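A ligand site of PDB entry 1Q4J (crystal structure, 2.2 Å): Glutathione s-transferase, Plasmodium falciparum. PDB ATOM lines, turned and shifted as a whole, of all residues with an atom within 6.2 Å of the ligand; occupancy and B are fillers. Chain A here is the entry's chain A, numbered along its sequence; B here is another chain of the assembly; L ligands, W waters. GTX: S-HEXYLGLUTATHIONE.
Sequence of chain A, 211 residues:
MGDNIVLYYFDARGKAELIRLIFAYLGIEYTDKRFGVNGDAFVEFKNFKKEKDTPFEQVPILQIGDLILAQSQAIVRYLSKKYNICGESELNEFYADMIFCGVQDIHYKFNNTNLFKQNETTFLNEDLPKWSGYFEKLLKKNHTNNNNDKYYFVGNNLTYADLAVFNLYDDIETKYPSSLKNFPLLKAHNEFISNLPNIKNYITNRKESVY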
ATOM      1  N   TYR A   9     -31.008 -21.384   4.190  1.00  0.00           N
ATOM      2  CA  TYR A   9     -29.794 -20.656   3.893  1.00  0.00           C
ATOM      3  C   TYR A   9     -30.140 -19.317   3.315  1.00  0.00           C
ATOM      4  O   TYR A   9     -31.281 -19.010   3.166  1.00  0.00           O
ATOM      5  CB  TYR A   9     -28.953 -21.443   2.893  1.00  0.00           C
ATOM      6  CG  TYR A   9     -27.537 -20.927   2.740  1.00  0.00           C
ATOM      7  CD1 TYR A   9     -27.056 -20.562   1.488  1.00  0.00           C
ATOM      8  CD2 TYR A   9     -26.682 -20.814   3.830  1.00  0.00           C
ATOM      9  CE1 TYR A   9     -25.753 -20.115   1.324  1.00  0.00           C
ATOM     10  CE2 TYR A   9     -25.341 -20.336   3.687  1.00  0.00           C
ATOM     11  CZ  TYR A   9     -24.896 -20.012   2.434  1.00  0.00           C
ATOM     12  OH  TYR A   9     -23.607 -19.565   2.222  1.00  0.00           O
ATOM     13  N   PHE A  10     -29.136 -18.506   3.062  1.00  0.00           N
ATOM     14  CA  PHE A  10     -29.322 -17.228   2.382  1.00  0.00           C
ATOM     15  C   PHE A  10     -29.611 -17.497   0.908  1.00  0.00           C
ATOM     16  O   PHE A  10     -29.491 -18.623   0.448  1.00  0.00           O
ATOM     17  CB  PHE A  10     -28.117 -16.337   2.593  1.00  0.00           C
ATOM     18  CG  PHE A  10     -27.952 -15.925   4.026  1.00  0.00           C
ATOM     19  CD1 PHE A  10     -26.917 -16.438   4.803  1.00  0.00           C
ATOM     20  CD2 PHE A  10     -28.883 -15.094   4.615  1.00  0.00           C
ATOM     21  CE1 PHE A  10     -26.793 -16.083   6.154  1.00  0.00           C
ATOM     22  CE2 PHE A  10     -28.753 -14.743   5.954  1.00  0.00           C
ATOM     23  CZ  PHE A  10     -27.720 -15.255   6.721  1.00  0.00           C
ATOM     24  N   GLY A  14     -23.111 -20.500  -2.201  1.00  0.00           N
ATOM     25  CA  GLY A  14     -22.221 -20.583  -1.047  1.00  0.00           C
ATOM     26  C   GLY A  14     -22.140 -21.934  -0.380  1.00  0.00           C
ATOM     27  O   GLY A  14     -21.877 -22.944  -1.033  1.00  0.00           O
ATOM     28  N   LYS A  15     -22.426 -21.926   0.913  1.00  0.00           N
ATOM     29  CA  LYS A  15     -22.291 -23.086   1.781  1.00  0.00           C
ATOM     30  C   LYS A  15     -23.378 -24.126   1.644  1.00  0.00           C
ATOM     31  O   LYS A  15     -23.251 -25.228   2.194  1.00  0.00           O
ATOM     32  CB  LYS A  15     -22.230 -22.630   3.220  1.00  0.00           C
ATOM     33  CG  LYS A  15     -20.962 -21.915   3.570  1.00  0.00           C
ATOM     34  CD  LYS A  15     -19.861 -22.898   3.805  1.00  0.00           C
ATOM     35  CE  LYS A  15     -18.714 -22.247   4.538  1.00  0.00           C
ATOM     36  NZ  LYS A  15     -17.742 -23.274   4.879  1.00  0.00           N
ATOM     37  N   PHE A  45     -33.182 -13.662   8.709  1.00  0.00           N
ATOM     38  CA  PHE A  45     -32.369 -14.597   9.494  1.00  0.00           C
ATOM     39  C   PHE A  45     -32.572 -14.368  10.972  1.00  0.00           C
ATOM     40  O   PHE A  45     -32.611 -15.309  11.760  1.00  0.00           O
ATOM     41  CB  PHE A  45     -30.880 -14.481   9.149  1.00  0.00           C
ATOM     42  CG  PHE A  45     -30.014 -15.458   9.899  1.00  0.00           C
ATOM     43  CD1 PHE A  45     -28.826 -15.067  10.468  1.00  0.00           C
ATOM     44  CD2 PHE A  45     -30.399 -16.778  10.025  1.00  0.00           C
ATOM     45  CE1 PHE A  45     -28.045 -15.971  11.127  1.00  0.00           C
ATOM     46  CE2 PHE A  45     -29.629 -17.666  10.707  1.00  0.00           C
ATOM     47  CZ  PHE A  45     -28.443 -17.266  11.256  1.00  0.00           C
ATOM     48  N   LYS A  49     -33.894 -17.315  13.692  1.00  0.00           N
ATOM     49  CA  LYS A  49     -33.273 -17.767  14.938  1.00  0.00           C
ATOM     50  C   LYS A  49     -34.189 -17.643  16.167  1.00  0.00           C
ATOM     51  O   LYS A  49     -34.064 -18.423  17.119  1.00  0.00           O
ATOM     52  CB  LYS A  49     -31.984 -17.001  15.220  1.00  0.00           C
ATOM     53  CG  LYS A  49     -30.932 -17.166  14.153  1.00  0.00           C
ATOM     54  CD  LYS A  49     -29.675 -16.457  14.516  1.00  0.00           C
ATOM     55  CE  LYS A  49     -29.771 -14.969  14.277  1.00  0.00           C
ATOM     56  NZ  LYS A  49     -28.585 -14.262  14.834  1.00  0.00           N
ATOM     57  N   GLU A  57     -26.351 -20.571  15.861  1.00  0.00           N
ATOM     58  CA  GLU A  57     -26.953 -19.370  15.279  1.00  0.00           C
ATOM     59  C   GLU A  57     -26.400 -19.059  13.915  1.00  0.00           C
ATOM     60  O   GLU A  57     -26.233 -17.920  13.568  1.00  0.00           O
ATOM     61  CB  GLU A  57     -26.783 -18.183  16.191  1.00  0.00           C
ATOM     62  CG  GLU A  57     -27.373 -18.458  17.574  1.00  0.00           C
ATOM     63  CD  GLU A  57     -27.443 -17.230  18.424  1.00  0.00           C
ATOM     64  OE1 GLU A  57     -28.580 -16.807  18.769  1.00  0.00           O
ATOM     65  OE2 GLU A  57     -26.366 -16.707  18.763  1.00  0.00           O
ATOM     66  N   GLN A  58     -26.143 -20.089  13.140  1.00  0.00           N
ATOM     67  CA  GLN A  58     -25.707 -19.879  11.755  1.00  0.00           C
ATOM     68  C   GLN A  58     -26.387 -20.840  10.799  1.00  0.00           C
ATOM     69  O   GLN A  58     -26.856 -21.908  11.194  1.00  0.00           O
ATOM     70  CB  GLN A  58     -24.166 -20.053  11.666  1.00  0.00           C
ATOM     71  CG  GLN A  58     -23.407 -19.049  12.571  1.00  0.00           C
ATOM     72  CD  GLN A  58     -22.029 -18.636  12.067  1.00  0.00           C
ATOM     73  OE1 GLN A  58     -21.849 -17.475  11.654  1.00  0.00           O
ATOM     74  NE2 GLN A  58     -21.055 -19.550  12.139  1.00  0.00           N
ATOM     75  N   VAL A  59     -26.392 -20.476   9.528  1.00  0.00           N
ATOM     76  CA  VAL A  59     -26.884 -21.368   8.492  1.00  0.00           C
ATOM     77  C   VAL A  59     -25.711 -21.775   7.632  1.00  0.00           C
ATOM     78  O   VAL A  59     -24.681 -21.115   7.682  1.00  0.00           O
ATOM     79  CB  VAL A  59     -28.010 -20.660   7.686  1.00  0.00           C
ATOM     80  CG1 VAL A  59     -29.248 -20.591   8.544  1.00  0.00           C
ATOM     81  CG2 VAL A  59     -27.573 -19.288   7.268  1.00  0.00           C
ATOM     82  N   PRO A  60     -25.840 -22.819   6.812  1.00  0.00           N
ATOM     83  CA  PRO A  60     -27.041 -23.663   6.683  1.00  0.00           C
ATOM     84  C   PRO A  60     -27.538 -24.493   7.869  1.00  0.00           C
ATOM     85  O   PRO A  60     -26.764 -24.966   8.724  1.00  0.00           O
ATOM     86  CB  PRO A  60     -26.701 -24.625   5.545  1.00  0.00           C
ATOM     87  CG  PRO A  60     -25.235 -24.568   5.402  1.00  0.00           C
ATOM     88  CD  PRO A  60     -24.779 -23.189   5.846  1.00  0.00           C
ATOM     89  N   ALA A  70     -26.952 -28.678  11.887  1.00  0.00           N
ATOM     90  CA  ALA A  70     -26.165 -27.548  11.461  1.00  0.00           C
ATOM     91  C   ALA A  70     -24.815 -28.033  10.969  1.00  0.00           C
ATOM     92  O   ALA A  70     -24.478 -29.216  11.134  1.00  0.00           O
ATOM     93  CB  ALA A  70     -26.020 -26.569  12.556  1.00  0.00           C
ATOM     94  N   GLN A  71     -24.086 -27.099  10.373  1.00  0.00           N
ATOM     95  CA  GLN A  71     -22.739 -27.272   9.828  1.00  0.00           C
ATOM     96  C   GLN A  71     -22.747 -27.977   8.511  1.00  0.00           C
ATOM     97  O   GLN A  71     -22.934 -29.201   8.430  1.00  0.00           O
ATOM     98  CB  GLN A  71     -21.791 -27.947  10.825  1.00  0.00           C
ATOM     99  CG  GLN A  71     -21.472 -27.060  11.999  1.00  0.00           C
ATOM    100  CD  GLN A  71     -20.525 -25.930  11.686  1.00  0.00           C
ATOM    101  OE1 GLN A  71     -20.321 -25.057  12.518  1.00  0.00           O
ATOM    102  NE2 GLN A  71     -19.948 -25.919  10.483  1.00  0.00           N
ATOM    103  N   SER A  72     -22.529 -27.202   7.459  1.00  0.00           N
ATOM    104  CA  SER A  72     -22.624 -27.696   6.070  1.00  0.00           C
ATOM    105  C   SER A  72     -21.833 -28.937   5.829  1.00  0.00           C
ATOM    106  O   SER A  72     -22.352 -29.892   5.286  1.00  0.00           O
ATOM    107  CB  SER A  72     -22.195 -26.627   5.056  1.00  0.00           C
ATOM    108  OG  SER A  72     -20.910 -26.115   5.330  1.00  0.00           O
ATOM    109  N   GLN A  73     -20.592 -28.955   6.272  1.00  0.00           N
ATOM    110  CA  GLN A  73     -19.732 -30.123   6.033  1.00  0.00           C
ATOM    111  C   GLN A  73     -20.242 -31.376   6.687  1.00  0.00           C
ATOM    112  O   GLN A  73     -20.175 -32.442   6.106  1.00  0.00           O
ATOM    113  CB  GLN A  73     -18.320 -29.848   6.482  1.00  0.00           C
ATOM    114  CG  GLN A  73     -17.553 -29.014   5.494  1.00  0.00           C
ATOM    115  CD  GLN A  73     -17.419 -27.564   5.908  1.00  0.00           C
ATOM    116  OE1 GLN A  73     -17.205 -27.265   7.091  1.00  0.00           O
ATOM    117  NE2 GLN A  73     -17.502 -26.643   4.924  1.00  0.00           N
ATOM    118  N   ILE A  75     -23.319 -31.926   7.590  1.00  0.00           N
ATOM    119  CA  ILE A  75     -24.563 -32.308   6.923  1.00  0.00           C
ATOM    120  C   ILE A  75     -24.228 -33.109   5.672  1.00  0.00           C
ATOM    121  O   ILE A  75     -24.765 -34.218   5.475  1.00  0.00           O
ATOM    122  CB  ILE A  75     -25.421 -31.067   6.562  1.00  0.00           C
ATOM    123  CG1 ILE A  75     -25.911 -30.404   7.822  1.00  0.00           C
ATOM    124  CG2 ILE A  75     -26.653 -31.477   5.726  1.00  0.00           C
ATOM    125  CD1 ILE A  75     -26.296 -28.920   7.658  1.00  0.00           C
ATOM    126  N   ASN A 111     -13.340 -17.741  -3.402  1.00  0.00           N
ATOM    127  CA  ASN A 111     -14.329 -16.821  -2.861  1.00  0.00           C
ATOM    128  C   ASN A 111     -13.699 -15.530  -2.296  1.00  0.00           C
ATOM    129  O   ASN A 111     -14.231 -14.435  -2.503  1.00  0.00           O
ATOM    130  CB  ASN A 111     -15.203 -17.518  -1.794  1.00  0.00           C
ATOM    131  CG  ASN A 111     -16.152 -18.561  -2.412  1.00  0.00           C
ATOM    132  OD1 ASN A 111     -16.673 -18.362  -3.517  1.00  0.00           O
ATOM    133  ND2 ASN A 111     -16.352 -19.670  -1.725  1.00  0.00           N
ATOM    134  N   TYR A 211     -22.803 -15.276  -5.598  1.00  0.00           N
ATOM    135  CA  TYR A 211     -21.886 -16.336  -5.128  1.00  0.00           C
ATOM    136  C   TYR A 211     -22.738 -17.555  -4.748  1.00  0.00           C
ATOM    137  O   TYR A 211     -23.966 -17.433  -4.688  1.00  0.00           O
ATOM    138  CB  TYR A 211     -21.076 -15.859  -3.904  1.00  0.00           C
ATOM    139  CG  TYR A 211     -21.950 -15.621  -2.666  1.00  0.00           C
ATOM    140  CD1 TYR A 211     -22.807 -14.511  -2.593  1.00  0.00           C
ATOM    141  CD2 TYR A 211     -21.949 -16.508  -1.589  1.00  0.00           C
ATOM    142  CE1 TYR A 211     -23.635 -14.278  -1.470  1.00  0.00           C
ATOM    143  CE2 TYR A 211     -22.768 -16.309  -0.468  1.00  0.00           C
ATOM    144  CZ  TYR A 211     -23.613 -15.183  -0.408  1.00  0.00           C
ATOM    145  OH  TYR A 211     -24.416 -14.959   0.698  1.00  0.00           O
ATOM    146  OXT TYR A 211     -22.177 -18.631  -4.455  1.00  0.00           O
ATOM    147  N   PHE B 116     -21.065 -11.965   1.934  1.00  0.00           N
ATOM    148  CA  PHE B 116     -21.058 -13.389   2.331  1.00  0.00           C
ATOM    149  C   PHE B 116     -21.874 -13.696   3.598  1.00  0.00           C
ATOM    150  O   PHE B 116     -22.188 -14.857   3.870  1.00  0.00           O
ATOM    151  CB  PHE B 116     -19.616 -13.855   2.507  1.00  0.00           C
ATOM    152  CG  PHE B 116     -18.878 -14.032   1.211  1.00  0.00           C
ATOM    153  CD1 PHE B 116     -17.476 -13.996   1.188  1.00  0.00           C
ATOM    154  CD2 PHE B 116     -19.564 -14.254  -0.005  1.00  0.00           C
ATOM    155  CE1 PHE B 116     -16.782 -14.173  -0.025  1.00  0.00           C
ATOM    156  CE2 PHE B 116     -18.876 -14.427  -1.206  1.00  0.00           C
ATOM    157  CZ  PHE B 116     -17.483 -14.388  -1.226  1.00  0.00           C
ATOM    158  N   LYS B 117     -22.235 -12.657   4.338  1.00  0.00           N
ATOM    159  CA  LYS B 117     -22.905 -12.745   5.627  1.00  0.00           C
ATOM    160  C   LYS B 117     -22.008 -13.420   6.679  1.00  0.00           C
ATOM    161  O   LYS B 117     -22.479 -13.837   7.743  1.00  0.00           O
ATOM    162  CB  LYS B 117     -24.262 -13.443   5.497  1.00  0.00           C
ATOM    163  CG  LYS B 117     -25.084 -13.019   4.272  1.00  0.00           C
ATOM    164  CD  LYS B 117     -25.533 -11.613   4.424  1.00  0.00           C
ATOM    165  CE  LYS B 117     -26.323 -11.113   3.222  1.00  0.00           C
ATOM    166  NZ  LYS B 117     -26.551  -9.613   3.347  1.00  0.00           N
ATOM    167  N   GLN B 118     -20.715 -13.490   6.375  1.00  0.00           N
ATOM    168  CA  GLN B 118     -19.682 -14.189   7.184  1.00  0.00           C
ATOM    169  C   GLN B 118     -19.849 -14.186   8.736  1.00  0.00           C
ATOM    170  O   GLN B 118     -19.989 -15.245   9.375  1.00  0.00           O
ATOM    171  CB  GLN B 118     -18.298 -13.589   6.792  1.00  0.00           C
ATOM    172  CG  GLN B 118     -17.089 -14.197   7.483  1.00  0.00           C
ATOM    173  CD  GLN B 118     -16.604 -15.480   6.836  1.00  0.00           C
ATOM    174  OE1 GLN B 118     -16.093 -15.411   5.680  1.00  0.00           O
ATOM    175  NE2 GLN B 118     -16.721 -16.545   7.490  1.00  0.00           N
ATOM    176  N   ASN B 119     -19.784 -12.995   9.313  1.00  0.00           N
ATOM    177  CA  ASN B 119     -19.929 -12.788  10.755  1.00  0.00           C
ATOM    178  C   ASN B 119     -20.889 -11.591  10.947  1.00  0.00           C
ATOM    179  O   ASN B 119     -20.643 -10.683  11.727  1.00  0.00           O
ATOM    180  CB  ASN B 119     -18.557 -12.483  11.390  1.00  0.00           C
ATOM    181  CG  ASN B 119     -17.551 -13.632  11.185  1.00  0.00           C
ATOM    182  OD1 ASN B 119     -17.731 -14.730  11.722  1.00  0.00           O
ATOM    183  ND2 ASN B 119     -16.512 -13.387  10.398  1.00  0.00           N
ATOM    184  N   GLU B 120     -21.978 -11.641  10.176  1.00  0.00           N
ATOM    185  CA  GLU B 120     -22.865 -10.510  10.019  1.00  0.00           C
ATOM    186  C   GLU B 120     -23.417 -10.115  11.359  1.00  0.00           C
ATOM    187  O   GLU B 120     -23.472  -8.950  11.679  1.00  0.00           O
ATOM    188  CB  GLU B 120     -23.984 -10.874   9.051  1.00  0.00           C
ATOM    189  CG  GLU B 120     -25.000  -9.777   8.865  1.00  0.00           C
ATOM    190  CD  GLU B 120     -25.854  -9.998   7.631  1.00  0.00           C
ATOM    191  OE1 GLU B 120     -26.760 -10.858   7.694  1.00  0.00           O
ATOM    192  OE2 GLU B 120     -25.577  -9.356   6.606  1.00  0.00           O
ATOM    193  N   THR B 121     -23.789 -11.084  12.162  1.00  0.00           N
ATOM    194  CA  THR B 121     -24.322 -10.794  13.466  1.00  0.00           C
ATOM    195  C   THR B 121     -23.307 -10.084  14.368  1.00  0.00           C
ATOM    196  O   THR B 121     -23.672  -9.181  15.110  1.00  0.00           O
ATOM    197  CB  THR B 121     -24.883 -12.063  14.113  1.00  0.00           C
ATOM    198  OG1 THR B 121     -26.041 -12.467  13.382  1.00  0.00           O
ATOM    199  CG2 THR B 121     -25.464 -11.778  15.533  1.00  0.00           C
ATOM    200  N   THR B 122     -22.052 -10.501  14.302  1.00  0.00           N
ATOM    201  CA  THR B 122     -21.026  -9.937  15.150  1.00  0.00           C
ATOM    202  C   THR B 122     -20.772  -8.511  14.665  1.00  0.00           C
ATOM    203  O   THR B 122     -20.720  -7.613  15.464  1.00  0.00           O
ATOM    204  CB  THR B 122     -19.726 -10.771  15.064  1.00  0.00           C
ATOM    205  OG1 THR B 122     -19.936 -12.071  15.589  1.00  0.00           O
ATOM    206  CG2 THR B 122     -18.658 -10.204  15.983  1.00  0.00           C
HETATM  207  N1  GTX L   1     -18.873 -23.746   9.421  1.00  0.00           N
HETATM  208  CA1 GTX L   1     -20.212 -23.272   9.125  1.00  0.00           C
HETATM  209  C1  GTX L   1     -20.825 -24.097   8.038  1.00  0.00           C
HETATM  210  O11 GTX L   1     -20.056 -24.519   7.065  1.00  0.00           O
HETATM  211  O12 GTX L   1     -22.089 -24.431   8.067  1.00  0.00           O
HETATM  212  CB1 GTX L   1     -20.165 -21.775   8.797  1.00  0.00           C
HETATM  213  CG1 GTX L   1     -21.574 -21.207   8.695  1.00  0.00           C
HETATM  214  CD1 GTX L   1     -21.558 -19.709   8.499  1.00  0.00           C
HETATM  215  OE1 GTX L   1     -20.375 -19.015   8.427  1.00  0.00           O
HETATM  216  N2  GTX L   1     -22.753 -19.120   8.352  1.00  0.00           N
HETATM  217  CA2 GTX L   1     -22.975 -17.784   7.836  1.00  0.00           C
HETATM  218  C2  GTX L   1     -24.113 -17.194   8.624  1.00  0.00           C
HETATM  219  O2  GTX L   1     -25.064 -18.026   9.195  1.00  0.00           O
HETATM  220  CB2 GTX L   1     -23.331 -17.768   6.348  1.00  0.00           C
HETATM  221  SG2 GTX L   1     -22.115 -18.610   5.271  1.00  0.00           S
HETATM  222  C1S GTX L   1     -20.716 -17.463   5.503  1.00  0.00           C
HETATM  223  C2S GTX L   1     -19.475 -17.895   4.728  1.00  0.00           C
HETATM  224  C3S GTX L   1     -19.621 -17.545   3.267  1.00  0.00           C
HETATM  225  C4S GTX L   1     -18.960 -18.570   2.356  1.00  0.00           C
HETATM  226  C5S GTX L   1     -19.587 -18.585   0.958  1.00  0.00           C
HETATM  227  C6S GTX L   1     -18.673 -17.951  -0.077  1.00  0.00           C
HETATM  228  N3  GTX L   1     -24.124 -15.881   8.746  1.00  0.00           N
HETATM  229  CA3 GTX L   1     -25.159 -15.162   9.466  1.00  0.00           C
HETATM  230  C3  GTX L   1     -24.681 -14.550  10.744  1.00  0.00           C
HETATM  231  O31 GTX L   1     -25.518 -13.798  11.382  1.00  0.00           O
HETATM  232  O32 GTX L   1     -23.467 -14.701  11.257  1.00  0.00           O
HETATM  233  O   HOH W   1     -17.960 -19.321   7.802  1.00  0.00           O
HETATM  234  O   HOH W   2     -19.315 -27.272   8.517  1.00  0.00           O
HETATM  235  O   HOH W   3     -24.332 -24.157   9.784  1.00  0.00           O
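CE1 of Phe 10 touches N3 of the ligand, at 3.7 Å.
Gly 14 touches the ligand (CA to C5S, 3.9 Å).
Phe 45 touches the ligand.
Pro 60 touches the ligand (CD to O12, 3.7 Å).
Gln 73 touches the ligand.
ND2 of Asn 111 touches C6S of the ligand (3.3 Å).
Tyr 211 touches the ligand.
Phe 116 of chain B touches the ligand (O to C1S, 3.4 Å).
Gln 118 of chain B touches the ligand.
N of Glu 120 of chain B touches O32 of the ligand (3.6 Å).
Hydrophobic or aromatic side chains that line the ligand: Tyr 9, Phe 10, Phe 45, Val 59, Pro 60, Tyr 211 and Phe 116 of chain B.
Water W1 bridges an oxygen (OE1) of the ligand (2.5 Å) and the side-chain amide nitrogen of Gln 118 of chain B (3.1 Å).
Water W3 lies within hydrogen-bond range of the backbone carbonyl oxygen of Pro 60 (2.8 Å), an oxygen (O12) of the ligand (2.8 Å) and the backbone NH of Gln 71 (3.0 Å).
Water W2 lies within hydrogen-bond range of the side-chain amide nitrogen (NE2) of Gln 71, the side-chain amide oxygen (OE1) of Gln 73, an oxygen (O11) of the ligand and the backbone NH (N) of Ser 72.
NZ of Lys 49 is in hydrogen-bond range of OG1 of Thr 121 of chain B (3.4 Å).
OG of Ser 72 is in hydrogen-bond range of NE2 of Gln 73 (3.5 Å).
OE2 of Glu 120 of chain B is in salt-bridge range of NZ of Lys 117 of chain B (3.4 Å).
The side-chain hydroxyl (OH) of Tyr 9 is in hydrogen-bond range of the backbone NH (N) of Lys 15 (2.9 Å).
The side-chain amino group of Lys 15 lies close to the side-chain amide nitrogen of Gln 73 (3.4 Å).
OXT of Tyr 211 sits at hydrogen-bond distance from N of Gly 14.
An oxygen (O31) of the ligand sits close to the backbone NH of Thr 121 of chain B, at 3.3 Å.
The side-chain hydroxyl (OG1) of Thr 121 of chain B sits at hydrogen-bond distance from an oxygen (O31) of the ligand (2.5 Å).
An oxygen (O12) of the ligand is in hydrogen-bond range of the backbone NH (N) of Ser 72 (2.9 Å).
The side-chain hydroxyl (OG) of Ser 72 is in hydrogen-bond range of an oxygen (O11) of the ligand.
A nitrogen (N1) of the ligand sits close to the side-chain amide nitrogen of Gln 71 (2.6 Å).
The backbone NH (N) of Val 59 is in hydrogen-bond range of an oxygen (O2) of the ligand (2.8 Å).
A nitrogen (N2) of the ligand sits at hydrogen-bond distance from the backbone carbonyl oxygen (O) of Val 59, at 2.9 Å.
O of Lys 117 of chain B lies within hydrogen-bond range of N3 of the ligand (2.8 Å).
An oxygen (O32) of the ligand sits close to the side-chain amide oxygen (OE1) of Gln 58 (3.2 Å).
NZ of Lys 15 is in salt-bridge range of O11 of the ligand (3.4 Å).
SG2 of the ligand lies close to OH of Tyr 9, at 3.5 Å.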
